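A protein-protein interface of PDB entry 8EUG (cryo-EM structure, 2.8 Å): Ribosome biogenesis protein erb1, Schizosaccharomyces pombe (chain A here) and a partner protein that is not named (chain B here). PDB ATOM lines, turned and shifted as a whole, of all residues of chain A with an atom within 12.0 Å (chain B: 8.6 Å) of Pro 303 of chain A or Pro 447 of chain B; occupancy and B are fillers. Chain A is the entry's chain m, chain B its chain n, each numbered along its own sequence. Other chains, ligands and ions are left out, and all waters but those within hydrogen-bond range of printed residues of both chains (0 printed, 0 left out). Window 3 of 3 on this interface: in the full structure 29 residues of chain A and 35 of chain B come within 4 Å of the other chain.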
ATOM      1  N   HIS A 296      17.171  -8.196 -11.460  1.00  0.00           N
ATOM      2  CA  HIS A 296      18.186  -8.228 -12.506  1.00  0.00           C
ATOM      3  C   HIS A 296      19.250  -9.293 -12.257  1.00  0.00           C
ATOM      4  O   HIS A 296      20.396  -9.133 -12.689  1.00  0.00           O
ATOM      5  CB  HIS A 296      18.836  -6.852 -12.643  1.00  0.00           C
ATOM      6  CG  HIS A 296      17.859  -5.718 -12.608  1.00  0.00           C
ATOM      7  ND1 HIS A 296      17.418  -5.154 -11.431  1.00  0.00           N
ATOM      8  CD2 HIS A 296      17.236  -5.046 -13.604  1.00  0.00           C
ATOM      9  CE1 HIS A 296      16.566  -4.182 -11.703  1.00  0.00           C
ATOM     10  NE2 HIS A 296      16.437  -4.096 -13.015  1.00  0.00           N
ATOM     11  N   GLU A 297      18.885 -10.378 -11.571  1.00  0.00           N
ATOM     12  CA  GLU A 297      19.805 -11.475 -11.257  1.00  0.00           C
ATOM     13  C   GLU A 297      20.970 -10.992 -10.392  1.00  0.00           C
ATOM     14  O   GLU A 297      22.138 -11.290 -10.652  1.00  0.00           O
ATOM     15  CB  GLU A 297      20.306 -12.159 -12.534  1.00  0.00           C
ATOM     16  CG  GLU A 297      20.828 -13.574 -12.331  1.00  0.00           C
ATOM     17  CD  GLU A 297      21.260 -14.223 -13.631  1.00  0.00           C
ATOM     18  OE1 GLU A 297      20.927 -13.680 -14.705  1.00  0.00           O
ATOM     19  OE2 GLU A 297      21.934 -15.273 -13.581  1.00  0.00           O
ATOM     20  N   GLU A 298      20.641 -10.226  -9.355  1.00  0.00           N
ATOM     21  CA  GLU A 298      21.576  -9.889  -8.289  1.00  0.00           C
ATOM     22  C   GLU A 298      21.108 -10.585  -7.019  1.00  0.00           C
ATOM     23  O   GLU A 298      19.967 -10.393  -6.586  1.00  0.00           O
ATOM     24  CB  GLU A 298      21.674  -8.377  -8.081  1.00  0.00           C
ATOM     25  CG  GLU A 298      22.833  -7.724  -8.824  1.00  0.00           C
ATOM     26  CD  GLU A 298      22.502  -7.415 -10.269  1.00  0.00           C
ATOM     27  OE1 GLU A 298      21.323  -7.556 -10.648  1.00  0.00           O
ATOM     28  OE2 GLU A 298      23.422  -7.035 -11.024  1.00  0.00           O
ATOM     29  N   SER A 299      21.989 -11.381  -6.428  1.00  0.00           N
ATOM     30  CA  SER A 299      21.611 -12.283  -5.347  1.00  0.00           C
ATOM     31  C   SER A 299      22.804 -12.435  -4.409  1.00  0.00           C
ATOM     32  O   SER A 299      23.713 -11.599  -4.401  1.00  0.00           O
ATOM     33  CB  SER A 299      21.121 -13.625  -5.918  1.00  0.00           C
ATOM     34  OG  SER A 299      22.133 -14.255  -6.683  1.00  0.00           O
ATOM     35  N   TYR A 300      22.784 -13.498  -3.601  1.00  0.00           N
ATOM     36  CA  TYR A 300      23.822 -13.709  -2.595  1.00  0.00           C
ATOM     37  C   TYR A 300      25.209 -13.756  -3.227  1.00  0.00           C
ATOM     38  O   TYR A 300      26.161 -13.166  -2.703  1.00  0.00           O
ATOM     39  CB  TYR A 300      23.540 -14.999  -1.822  1.00  0.00           C
ATOM     40  CG  TYR A 300      22.240 -14.998  -1.042  1.00  0.00           C
ATOM     41  CD1 TYR A 300      21.569 -13.813  -0.766  1.00  0.00           C
ATOM     42  CD2 TYR A 300      21.683 -16.186  -0.587  1.00  0.00           C
ATOM     43  CE1 TYR A 300      20.380 -13.813  -0.056  1.00  0.00           C
ATOM     44  CE2 TYR A 300      20.495 -16.195   0.124  1.00  0.00           C
ATOM     45  CZ  TYR A 300      19.849 -15.006   0.386  1.00  0.00           C
ATOM     46  OH  TYR A 300      18.668 -15.011   1.094  1.00  0.00           O
ATOM     47  N   ASN A 301      25.344 -14.457  -4.353  1.00  0.00           N
ATOM     48  CA  ASN A 301      26.635 -14.558  -5.023  1.00  0.00           C
ATOM     49  C   ASN A 301      26.473 -14.858  -6.511  1.00  0.00           C
ATOM     50  O   ASN A 301      26.738 -15.985  -6.951  1.00  0.00           O
ATOM     51  CB  ASN A 301      27.497 -15.631  -4.352  1.00  0.00           C
ATOM     52  CG  ASN A 301      26.751 -16.938  -4.153  1.00  0.00           C
ATOM     53  OD1 ASN A 301      25.556 -16.944  -3.858  1.00  0.00           O
ATOM     54  ND2 ASN A 301      27.455 -18.053  -4.318  1.00  0.00           N
ATOM     55  N   PRO A 302      26.053 -13.886  -7.316  1.00  0.00           N
ATOM     56  CA  PRO A 302      25.939 -14.117  -8.754  1.00  0.00           C
ATOM     57  C   PRO A 302      27.245 -13.803  -9.459  1.00  0.00           C
ATOM     58  O   PRO A 302      28.014 -12.939  -9.010  1.00  0.00           O
ATOM     59  CB  PRO A 302      24.829 -13.143  -9.169  1.00  0.00           C
ATOM     60  CG  PRO A 302      25.016 -11.987  -8.241  1.00  0.00           C
ATOM     61  CD  PRO A 302      25.560 -12.550  -6.937  1.00  0.00           C
ATOM     62  N   PRO A 303      27.539 -14.487 -10.566  1.00  0.00           N
ATOM     63  CA  PRO A 303      28.786 -14.217 -11.290  1.00  0.00           C
ATOM     64  C   PRO A 303      28.641 -13.100 -12.311  1.00  0.00           C
ATOM     65  O   PRO A 303      29.519 -12.908 -13.158  1.00  0.00           O
ATOM     66  CB  PRO A 303      29.082 -15.561 -11.964  1.00  0.00           C
ATOM     67  CG  PRO A 303      27.714 -16.154 -12.215  1.00  0.00           C
ATOM     68  CD  PRO A 303      26.737 -15.528 -11.233  1.00  0.00           C
ATOM     69  N   GLU A 304      27.539 -12.357 -12.240  1.00  0.00           N
ATOM     70  CA  GLU A 304      27.272 -11.281 -13.191  1.00  0.00           C
ATOM     71  C   GLU A 304      28.279 -10.145 -13.044  1.00  0.00           C
ATOM     72  O   GLU A 304      28.853  -9.682 -14.030  1.00  0.00           O
ATOM     73  CB  GLU A 304      25.850 -10.746 -13.008  1.00  0.00           C
ATOM     74  CG  GLU A 304      25.405  -9.772 -14.091  1.00  0.00           C
ATOM     75  CD  GLU A 304      25.858 -10.191 -15.478  1.00  0.00           C
ATOM     76  OE1 GLU A 304      25.317 -11.186 -16.003  1.00  0.00           O
ATOM     77  OE2 GLU A 304      26.751  -9.524 -16.042  1.00  0.00           O
ATOM     78  N   PHE B 181      11.639 -15.465  -5.084  1.00  0.00           N
ATOM     79  CA  PHE B 181      13.039 -15.161  -5.340  1.00  0.00           C
ATOM     80  C   PHE B 181      13.611 -14.342  -4.191  1.00  0.00           C
ATOM     81  O   PHE B 181      12.925 -13.486  -3.625  1.00  0.00           O
ATOM     82  CB  PHE B 181      13.197 -14.403  -6.663  1.00  0.00           C
ATOM     83  CG  PHE B 181      14.574 -13.849  -6.888  1.00  0.00           C
ATOM     84  CD1 PHE B 181      15.618 -14.677  -7.260  1.00  0.00           C
ATOM     85  CD2 PHE B 181      14.822 -12.495  -6.736  1.00  0.00           C
ATOM     86  CE1 PHE B 181      16.884 -14.165  -7.469  1.00  0.00           C
ATOM     87  CE2 PHE B 181      16.086 -11.980  -6.944  1.00  0.00           C
ATOM     88  CZ  PHE B 181      17.118 -12.816  -7.311  1.00  0.00           C
ATOM     89  N   GLN B 422      18.111 -22.368   0.721  1.00  0.00           N
ATOM     90  CA  GLN B 422      18.032 -22.260  -0.731  1.00  0.00           C
ATOM     91  C   GLN B 422      17.641 -23.580  -1.385  1.00  0.00           C
ATOM     92  O   GLN B 422      17.135 -23.575  -2.513  1.00  0.00           O
ATOM     93  CB  GLN B 422      19.367 -21.759  -1.289  1.00  0.00           C
ATOM     94  CG  GLN B 422      19.352 -21.457  -2.780  1.00  0.00           C
ATOM     95  CD  GLN B 422      20.504 -20.573  -3.211  1.00  0.00           C
ATOM     96  OE1 GLN B 422      21.239 -20.041  -2.379  1.00  0.00           O
ATOM     97  NE2 GLN B 422      20.667 -20.411  -4.518  1.00  0.00           N
ATOM     98  N   ASP B 426      15.115 -23.580  -4.540  1.00  0.00           N
ATOM     99  CA  ASP B 426      15.488 -24.153  -5.829  1.00  0.00           C
ATOM    100  C   ASP B 426      14.590 -25.332  -6.177  1.00  0.00           C
ATOM    101  O   ASP B 426      14.345 -25.613  -7.357  1.00  0.00           O
ATOM    102  CB  ASP B 426      16.961 -24.563  -5.821  1.00  0.00           C
ATOM    103  CG  ASP B 426      17.892 -23.385  -6.042  1.00  0.00           C
ATOM    104  OD1 ASP B 426      17.489 -22.436  -6.748  1.00  0.00           O
ATOM    105  OD2 ASP B 426      19.026 -23.406  -5.521  1.00  0.00           O
ATOM    106  N   LYS B 430      12.190 -25.380  -9.604  1.00  0.00           N
ATOM    107  CA  LYS B 430      12.364 -26.488 -10.534  1.00  0.00           C
ATOM    108  C   LYS B 430      11.194 -27.460 -10.534  1.00  0.00           C
ATOM    109  O   LYS B 430      11.124 -28.318 -11.421  1.00  0.00           O
ATOM    110  CB  LYS B 430      13.652 -27.257 -10.214  1.00  0.00           C
ATOM    111  CG  LYS B 430      14.892 -26.754 -10.943  1.00  0.00           C
ATOM    112  CD  LYS B 430      15.463 -25.498 -10.306  1.00  0.00           C
ATOM    113  CE  LYS B 430      16.789 -25.109 -10.946  1.00  0.00           C
ATOM    114  NZ  LYS B 430      17.349 -23.851 -10.377  1.00  0.00           N
ATOM    115  N   LEU B 438      24.352 -30.851  -2.550  1.00  0.00           N
ATOM    116  CA  LEU B 438      24.687 -29.513  -3.031  1.00  0.00           C
ATOM    117  C   LEU B 438      24.480 -28.462  -1.948  1.00  0.00           C
ATOM    118  O   LEU B 438      25.284 -27.533  -1.809  1.00  0.00           O
ATOM    119  CB  LEU B 438      23.849 -29.178  -4.264  1.00  0.00           C
ATOM    120  CG  LEU B 438      24.211 -27.883  -4.990  1.00  0.00           C
ATOM    121  CD1 LEU B 438      25.605 -27.977  -5.590  1.00  0.00           C
ATOM    122  CD2 LEU B 438      23.178 -27.571  -6.059  1.00  0.00           C
ATOM    123  N   TYR B 439      23.406 -28.591  -1.169  1.00  0.00           N
ATOM    124  CA  TYR B 439      22.998 -27.577  -0.205  1.00  0.00           C
ATOM    125  C   TYR B 439      23.050 -28.096   1.229  1.00  0.00           C
ATOM    126  O   TYR B 439      22.246 -27.694   2.072  1.00  0.00           O
ATOM    127  CB  TYR B 439      21.602 -27.060  -0.547  1.00  0.00           C
ATOM    128  CG  TYR B 439      21.591 -26.144  -1.749  1.00  0.00           C
ATOM    129  CD1 TYR B 439      22.613 -25.229  -1.953  1.00  0.00           C
ATOM    130  CD2 TYR B 439      20.587 -26.226  -2.703  1.00  0.00           C
ATOM    131  CE1 TYR B 439      22.615 -24.394  -3.050  1.00  0.00           C
ATOM    132  CE2 TYR B 439      20.583 -25.398  -3.809  1.00  0.00           C
ATOM    133  CZ  TYR B 439      21.601 -24.484  -3.978  1.00  0.00           C
ATOM    134  OH  TYR B 439      21.602 -23.656  -5.078  1.00  0.00           O
ATOM    135  N   THR B 444      28.972 -25.562  -0.628  1.00  0.00           N
ATOM    136  CA  THR B 444      29.034 -24.508  -1.627  1.00  0.00           C
ATOM    137  C   THR B 444      27.635 -24.142  -2.116  1.00  0.00           C
ATOM    138  O   THR B 444      26.687 -24.928  -2.025  1.00  0.00           O
ATOM    139  CB  THR B 444      29.910 -24.935  -2.806  1.00  0.00           C
ATOM    140  OG1 THR B 444      30.108 -23.820  -3.686  1.00  0.00           O
ATOM    141  CG2 THR B 444      29.263 -26.078  -3.568  1.00  0.00           C
ATOM    142  N   LEU B 445      27.517 -22.929  -2.645  1.00  0.00           N
ATOM    143  CA  LEU B 445      26.229 -22.376  -3.065  1.00  0.00           C
ATOM    144  C   LEU B 445      26.320 -21.962  -4.525  1.00  0.00           C
ATOM    145  O   LEU B 445      27.002 -20.964  -4.839  1.00  0.00           O
ATOM    146  CB  LEU B 445      25.824 -21.180  -2.206  1.00  0.00           C
ATOM    147  CG  LEU B 445      25.143 -21.361  -0.841  1.00  0.00           C
ATOM    148  CD1 LEU B 445      23.645 -21.584  -0.997  1.00  0.00           C
ATOM    149  CD2 LEU B 445      25.774 -22.456   0.001  1.00  0.00           C
ATOM    150  N   PRO B 446      25.684 -22.687  -5.444  1.00  0.00           N
ATOM    151  CA  PRO B 446      25.626 -22.218  -6.825  1.00  0.00           C
ATOM    152  C   PRO B 446      24.905 -20.891  -6.903  1.00  0.00           C
ATOM    153  O   PRO B 446      24.024 -20.589  -6.073  1.00  0.00           O
ATOM    154  CB  PRO B 446      24.844 -23.328  -7.541  1.00  0.00           C
ATOM    155  CG  PRO B 446      25.075 -24.543  -6.726  1.00  0.00           C
ATOM    156  CD  PRO B 446      25.224 -24.080  -5.305  1.00  0.00           C
ATOM    157  N   PRO B 447      25.249 -20.047  -7.889  1.00  0.00           N
ATOM    158  CA  PRO B 447      24.653 -18.705  -7.967  1.00  0.00           C
ATOM    159  C   PRO B 447      23.133 -18.720  -7.998  1.00  0.00           C
ATOM    160  O   PRO B 447      22.522 -19.344  -8.873  1.00  0.00           O
ATOM    161  CB  PRO B 447      25.232 -18.140  -9.271  1.00  0.00           C
ATOM    162  CG  PRO B 447      26.493 -18.903  -9.491  1.00  0.00           C
ATOM    163  CD  PRO B 447      26.229 -20.282  -8.965  1.00  0.00           C
ATOM    164  N   HIS B 448      22.520 -18.043  -7.030  1.00  0.00           N
ATOM    165  CA  HIS B 448      21.068 -17.958  -6.960  1.00  0.00           C
ATOM    166  C   HIS B 448      20.524 -17.254  -8.197  1.00  0.00           C
ATOM    167  O   HIS B 448      20.790 -16.069  -8.416  1.00  0.00           O
ATOM    168  CB  HIS B 448      20.654 -17.221  -5.688  1.00  0.00           C
ATOM    169  CG  HIS B 448      19.182 -17.253  -5.417  1.00  0.00           C
ATOM    170  ND1 HIS B 448      18.520 -18.398  -5.028  1.00  0.00           N
ATOM    171  CD2 HIS B 448      18.246 -16.276  -5.460  1.00  0.00           C
ATOM    172  CE1 HIS B 448      17.239 -18.128  -4.857  1.00  0.00           C
ATOM    173  NE2 HIS B 448      17.046 -16.847  -5.112  1.00  0.00           N
ATOM    174  N   LEU B 449      19.762 -17.989  -9.002  1.00  0.00           N
ATOM    175  CA  LEU B 449      19.263 -17.499 -10.277  1.00  0.00           C
ATOM    176  C   LEU B 449      17.861 -16.931 -10.113  1.00  0.00           C
ATOM    177  O   LEU B 449      17.029 -17.493  -9.394  1.00  0.00           O
ATOM    178  CB  LEU B 449      19.250 -18.618 -11.321  1.00  0.00           C
ATOM    179  CG  LEU B 449      20.601 -19.234 -11.685  1.00  0.00           C
ATOM    180  CD1 LEU B 449      20.425 -20.360 -12.693  1.00  0.00           C
ATOM    181  CD2 LEU B 449      21.551 -18.175 -12.217  1.00  0.00           C
ATOM    182  N   SER B 450      17.604 -15.812 -10.786  1.00  0.00           N
ATOM    183  CA  SER B 450      16.295 -15.178 -10.740  1.00  0.00           C
ATOM    184  C   SER B 450      15.397 -15.775 -11.814  1.00  0.00           C
ATOM    185  O   SER B 450      15.719 -15.662 -13.005  1.00  0.00           O
ATOM    186  CB  SER B 450      16.417 -13.677 -10.941  1.00  0.00           C
ATOM    187  OG  SER B 450      15.143 -13.056 -10.929  1.00  0.00           O
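OG of Ser 299 of chain A sits at hydrogen-bond distance from O of His 448 of chain B, 2.8 Å away.
ND2 of Asn 301 of chain A sits at hydrogen-bond distance from O of Leu 445 of chain B, 3.0 Å away.
Of the printed residues of chain B, Pro 303 of chain A touches Pro 447.
Pro 447 of chain B touches two residues of chain A.
His 448 of chain B touches one residue of chain A.
Leu 449 of chain B touches just one residue of chain A: Glu 297 (3.2 Å).
Of the printed residues of chain B, Glu 297 of chain A touches Leu 449.
Of the printed residues of chain B, Ser 299 of chain A touches His 448 (2.8 Å).
Of the printed residues of chain A, Phe 181 of chain B touches Glu 298.
Printed residues of chain B within 4 Å of Asn 301 of chain A: Leu 445 (3.0 Å) and Pro 447 (3.5 Å).
Ser 450 of chain B touches none of the printed residues of chain A.
The backbone carbonyl oxygen (O) of His 296 of chain A lies close to the side-chain carboxylate (OE1) of Glu 298 of chain A (2.7 Å).
NE2 of Gln 422 of chain B lies within hydrogen-bond range of ND1 of His 448 of chain B (3.0 Å).
OE2 of Glu 297 of chain A touches CD2 of Leu 449 of chain B, 3.2 Å away.
Glu 298 of chain A touches Phe 181 of chain B (O to CZ, 3.8 Å).
Asn 301 of chain A touches Pro 447 of chain B.
CB of Pro 447 of chain B touches CD of Pro 303 of chain A, 3.6 Å away.
Of the 13 printed residues of chain B, 5 touch a printed residue of chain A.
Hydrophobic or aromatic side chains of chain B within 4 Å of the printed part of chain A: Phe 181, Pro 447, His 448 and Leu 449.
Of the 9 printed residues of chain A, 5 touch a printed residue of chain B.
Among the printed residues, no Asp or Glu carboxylate lies within 4 Å of a Lys or Arg side-chain nitrogen of the other chain.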
